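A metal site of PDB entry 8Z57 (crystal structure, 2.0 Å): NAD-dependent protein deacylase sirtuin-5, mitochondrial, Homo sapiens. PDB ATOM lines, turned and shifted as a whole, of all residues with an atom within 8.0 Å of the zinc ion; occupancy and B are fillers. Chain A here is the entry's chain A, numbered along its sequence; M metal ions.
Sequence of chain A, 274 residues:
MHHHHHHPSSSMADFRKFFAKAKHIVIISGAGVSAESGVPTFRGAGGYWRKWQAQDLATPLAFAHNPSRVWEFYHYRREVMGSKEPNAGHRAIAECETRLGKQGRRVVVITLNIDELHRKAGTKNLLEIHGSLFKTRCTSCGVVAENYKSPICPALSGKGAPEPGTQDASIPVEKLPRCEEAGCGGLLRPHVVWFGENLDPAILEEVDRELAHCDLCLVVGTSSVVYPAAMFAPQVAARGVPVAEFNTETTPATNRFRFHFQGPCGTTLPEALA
The zinc ion is bound by the side-chain sulfur (SG) of Cys 141, the side-chain sulfur (SG) of Cys 184, the side-chain sulfur (SG) of Cys 138 and the side-chain sulfur (SG) of Cys 179.
The zinc ion has four donor atoms within binding distance.
The backbone NH (N) of Cys 179 sits at hydrogen-bond distance from the backbone carbonyl oxygen (O) of Gly 186, at 2.8 Å.
The side-chain sulfur (SG) of Cys 141 lies close to the backbone NH (N) of Val 143, at 3.6 Å.
SG of Cys 138 lies close to N of Ser 140, 3.3 Å away.
N of Glu 181 lies close to SG of Cys 179, 3.5 Å away.
O of Cys 179 sits close to N of Gly 185, at 3.2 Å.
N of Gly 186 lies close to SG of Cys 184 (3.4 Å).
The backbone NH (N) of Cys 138 sits at hydrogen-bond distance from the backbone carbonyl oxygen (O) of Val 143 (3.1 Å).
Of the 19 residues printed, 4 come within 4 Å of the zinc ion.
The nearest printed residue that does not touch the zinc ion is Gly 186 (4.5 Å).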
ATOM      1  N   ARG A 137     -31.422  24.817  11.359  1.00  0.00           N
ATOM      2  CA  ARG A 137     -30.997  25.891  10.497  1.00  0.00           C
ATOM      3  C   ARG A 137     -30.038  26.770  11.283  1.00  0.00           C
ATOM      4  O   ARG A 137     -30.271  27.030  12.472  1.00  0.00           O
ATOM      5  CB  ARG A 137     -32.186  26.753  10.021  1.00  0.00           C
ATOM      6  CG  ARG A 137     -31.739  27.922   9.180  1.00  0.00           C
ATOM      7  CD  ARG A 137     -32.832  28.442   8.257  1.00  0.00           C
ATOM      8  NE  ARG A 137     -33.643  29.455   8.913  1.00  0.00           N
ATOM      9  CZ  ARG A 137     -34.851  29.234   9.414  1.00  0.00           C
ATOM     10  NH1 ARG A 137     -35.363  28.020   9.337  1.00  0.00           N
ATOM     11  NH2 ARG A 137     -35.549  30.205   9.985  1.00  0.00           N
ATOM     12  N   CYS A 138     -28.989  27.229  10.617  1.00  0.00           N
ATOM     13  CA  CYS A 138     -27.997  28.062  11.282  1.00  0.00           C
ATOM     14  C   CYS A 138     -28.408  29.515  11.234  1.00  0.00           C
ATOM     15  O   CYS A 138     -28.695  30.059  10.155  1.00  0.00           O
ATOM     16  CB  CYS A 138     -26.631  27.890  10.616  1.00  0.00           C
ATOM     17  SG  CYS A 138     -25.416  28.988  11.332  1.00  0.00           S
ATOM     18  N   THR A 139     -28.430  30.162  12.400  1.00  0.00           N
ATOM     19  CA  THR A 139     -28.874  31.552  12.472  1.00  0.00           C
ATOM     20  C   THR A 139     -27.869  32.523  11.870  1.00  0.00           C
ATOM     21  O   THR A 139     -28.162  33.724  11.808  1.00  0.00           O
ATOM     22  CB  THR A 139     -29.215  31.956  13.913  1.00  0.00           C
ATOM     23  OG1 THR A 139     -28.067  31.843  14.752  1.00  0.00           O
ATOM     24  CG2 THR A 139     -30.369  31.109  14.457  1.00  0.00           C
ATOM     25  N   SER A 140     -26.703  32.041  11.456  1.00  0.00           N
ATOM     26  CA  SER A 140     -25.666  32.874  10.854  1.00  0.00           C
ATOM     27  C   SER A 140     -25.565  32.678   9.355  1.00  0.00           C
ATOM     28  O   SER A 140     -25.656  33.648   8.594  1.00  0.00           O
ATOM     29  CB  SER A 140     -24.302  32.602  11.513  1.00  0.00           C
ATOM     30  OG  SER A 140     -24.199  33.203  12.798  1.00  0.00           O
ATOM     31  N   CYS A 141     -25.371  31.442   8.896  1.00  0.00           N
ATOM     32  CA  CYS A 141     -25.181  31.167   7.476  1.00  0.00           C
ATOM     33  C   CYS A 141     -26.447  30.699   6.768  1.00  0.00           C
ATOM     34  O   CYS A 141     -26.485  30.699   5.542  1.00  0.00           O
ATOM     35  CB  CYS A 141     -24.029  30.165   7.282  1.00  0.00           C
ATOM     36  SG  CYS A 141     -24.440  28.471   7.733  1.00  0.00           S
ATOM     37  N   GLY A 142     -27.482  30.291   7.521  1.00  0.00           N
ATOM     38  CA  GLY A 142     -28.737  29.865   6.935  1.00  0.00           C
ATOM     39  C   GLY A 142     -28.802  28.407   6.495  1.00  0.00           C
ATOM     40  O   GLY A 142     -29.882  27.958   6.088  1.00  0.00           O
ATOM     41  N   VAL A 143     -27.701  27.663   6.573  1.00  0.00           N
ATOM     42  CA  VAL A 143     -27.680  26.297   6.065  1.00  0.00           C
ATOM     43  C   VAL A 143     -28.653  25.419   6.848  1.00  0.00           C
ATOM     44  O   VAL A 143     -28.762  25.512   8.084  1.00  0.00           O
ATOM     45  CB  VAL A 143     -26.243  25.760   6.125  1.00  0.00           C
ATOM     46  CG1 VAL A 143     -26.228  24.237   6.107  1.00  0.00           C
ATOM     47  CG2 VAL A 143     -25.439  26.302   4.952  1.00  0.00           C
ATOM     48  N   VAL A 144     -29.387  24.569   6.125  1.00  0.00           N
ATOM     49  CA  VAL A 144     -30.352  23.656   6.716  1.00  0.00           C
ATOM     50  C   VAL A 144     -29.782  22.253   6.641  1.00  0.00           C
ATOM     51  O   VAL A 144     -29.239  21.852   5.606  1.00  0.00           O
ATOM     52  CB  VAL A 144     -31.709  23.727   5.983  1.00  0.00           C
ATOM     53  CG1 VAL A 144     -32.692  22.740   6.604  1.00  0.00           C
ATOM     54  CG2 VAL A 144     -32.252  25.120   6.072  1.00  0.00           C
ATOM     55  N   ARG A 178     -24.476  23.843  17.474  1.00  0.00           N
ATOM     56  CA  ARG A 178     -23.652  24.789  16.739  1.00  0.00           C
ATOM     57  C   ARG A 178     -23.498  24.320  15.294  1.00  0.00           C
ATOM     58  O   ARG A 178     -23.414  23.115  15.035  1.00  0.00           O
ATOM     59  CB  ARG A 178     -22.275  24.836  17.405  1.00  0.00           C
ATOM     60  CG  ARG A 178     -21.693  26.192  17.581  1.00  0.00           C
ATOM     61  CD  ARG A 178     -22.583  27.100  18.393  1.00  0.00           C
ATOM     62  NE  ARG A 178     -22.321  28.468  17.974  1.00  0.00           N
ATOM     63  CZ  ARG A 178     -22.755  29.543  18.598  1.00  0.00           C
ATOM     64  NH1 ARG A 178     -23.508  29.437  19.678  1.00  0.00           N
ATOM     65  NH2 ARG A 178     -22.439  30.729  18.113  1.00  0.00           N
ATOM     66  N   CYS A 179     -23.469  25.266  14.362  1.00  0.00           N
ATOM     67  CA  CYS A 179     -23.242  24.941  12.959  1.00  0.00           C
ATOM     68  C   CYS A 179     -21.880  24.294  12.758  1.00  0.00           C
ATOM     69  O   CYS A 179     -20.843  24.873  13.135  1.00  0.00           O
ATOM     70  CB  CYS A 179     -23.328  26.208  12.118  1.00  0.00           C
ATOM     71  SG  CYS A 179     -23.297  25.934  10.329  1.00  0.00           S
ATOM     72  N   GLU A 180     -21.854  23.107  12.162  1.00  0.00           N
ATOM     73  CA  GLU A 180     -20.602  22.427  11.862  1.00  0.00           C
ATOM     74  C   GLU A 180     -20.060  22.750  10.464  1.00  0.00           C
ATOM     75  O   GLU A 180     -19.044  22.177  10.069  1.00  0.00           O
ATOM     76  CB  GLU A 180     -20.741  20.905  12.046  1.00  0.00           C
ATOM     77  CG  GLU A 180     -20.078  20.391  13.325  1.00  0.00           C
ATOM     78  CD  GLU A 180     -20.934  19.357  14.052  1.00  0.00           C
ATOM     79  OE1 GLU A 180     -21.010  19.429  15.295  1.00  0.00           O
ATOM     80  OE2 GLU A 180     -21.510  18.487  13.375  1.00  0.00           O
ATOM     81  N   GLU A 181     -20.716  23.650   9.735  1.00  0.00           N
ATOM     82  CA  GLU A 181     -20.207  24.071   8.440  1.00  0.00           C
ATOM     83  C   GLU A 181     -18.824  24.686   8.630  1.00  0.00           C
ATOM     84  O   GLU A 181     -18.622  25.494   9.541  1.00  0.00           O
ATOM     85  CB  GLU A 181     -21.143  25.100   7.816  1.00  0.00           C
ATOM     86  CG  GLU A 181     -21.461  24.903   6.338  1.00  0.00           C
ATOM     87  CD  GLU A 181     -21.894  23.486   6.028  1.00  0.00           C
ATOM     88  OE1 GLU A 181     -21.404  22.905   5.028  1.00  0.00           O
ATOM     89  OE2 GLU A 181     -22.721  22.936   6.792  1.00  0.00           O
ATOM     90  N   ALA A 182     -17.883  24.302   7.771  1.00  0.00           N
ATOM     91  CA  ALA A 182     -16.528  24.807   7.875  1.00  0.00           C
ATOM     92  C   ALA A 182     -16.524  26.319   7.990  1.00  0.00           C
ATOM     93  O   ALA A 182     -16.987  27.031   7.099  1.00  0.00           O
ATOM     94  CB  ALA A 182     -15.732  24.367   6.638  1.00  0.00           C
ATOM     95  N   GLY A 183     -16.035  26.809   9.132  1.00  0.00           N
ATOM     96  CA  GLY A 183     -15.834  28.223   9.333  1.00  0.00           C
ATOM     97  C   GLY A 183     -17.015  28.990   9.888  1.00  0.00           C
ATOM     98  O   GLY A 183     -16.880  30.201  10.109  1.00  0.00           O
ATOM     99  N   CYS A 184     -18.169  28.351  10.118  1.00  0.00           N
ATOM    100  CA  CYS A 184     -19.280  29.126  10.657  1.00  0.00           C
ATOM    101  C   CYS A 184     -19.380  29.033  12.171  1.00  0.00           C
ATOM    102  O   CYS A 184     -19.022  29.974  12.889  1.00  0.00           O
ATOM    103  CB  CYS A 184     -20.597  28.660  10.018  1.00  0.00           C
ATOM    104  SG  CYS A 184     -22.041  29.542  10.617  1.00  0.00           S
ATOM    105  N   GLY A 185     -19.752  27.865  12.688  1.00  0.00           N
ATOM    106  CA  GLY A 185     -19.951  27.700  14.108  1.00  0.00           C
ATOM    107  C   GLY A 185     -21.033  28.550  14.735  1.00  0.00           C
ATOM    108  O   GLY A 185     -21.036  28.727  15.958  1.00  0.00           O
ATOM    109  N   GLY A 186     -21.960  29.073  13.945  1.00  0.00           N
ATOM    110  CA  GLY A 186     -23.055  29.854  14.486  1.00  0.00           C
ATOM    111  C   GLY A 186     -24.075  29.025  15.243  1.00  0.00           C
ATOM    112  O   GLY A 186     -24.041  27.796  15.293  1.00  0.00           O
ATOM    113  N   LEU A 187     -25.015  29.735  15.861  1.00  0.00           N
ATOM    114  CA  LEU A 187     -26.021  29.109  16.711  1.00  0.00           C
ATOM    115  C   LEU A 187     -27.128  28.498  15.853  1.00  0.00           C
ATOM    116  O   LEU A 187     -27.705  29.179  14.999  1.00  0.00           O
ATOM    117  CB  LEU A 187     -26.624  30.162  17.642  1.00  0.00           C
ATOM    118  CG  LEU A 187     -27.828  29.689  18.467  1.00  0.00           C
ATOM    119  CD1 LEU A 187     -27.435  28.524  19.376  1.00  0.00           C
ATOM    120  CD2 LEU A 187     -28.435  30.828  19.285  1.00  0.00           C
ATOM    121  N   LEU A 188     -27.420  27.230  16.102  1.00  0.00           N
ATOM    122  CA  LEU A 188     -28.506  26.553  15.389  1.00  0.00           C
ATOM    123  C   LEU A 188     -29.841  26.780  16.079  1.00  0.00           C
ATOM    124  O   LEU A 188     -29.929  26.868  17.312  1.00  0.00           O
ATOM    125  CB  LEU A 188     -28.261  25.040  15.300  1.00  0.00           C
ATOM    126  CG  LEU A 188     -27.057  24.621  14.465  1.00  0.00           C
ATOM    127  CD1 LEU A 188     -27.034  23.099  14.254  1.00  0.00           C
ATOM    128  CD2 LEU A 188     -27.069  25.345  13.126  1.00  0.00           C
HETATM  129 ZN    ZN M   1     -23.726  28.252   9.857  1.00  0.00          ZN
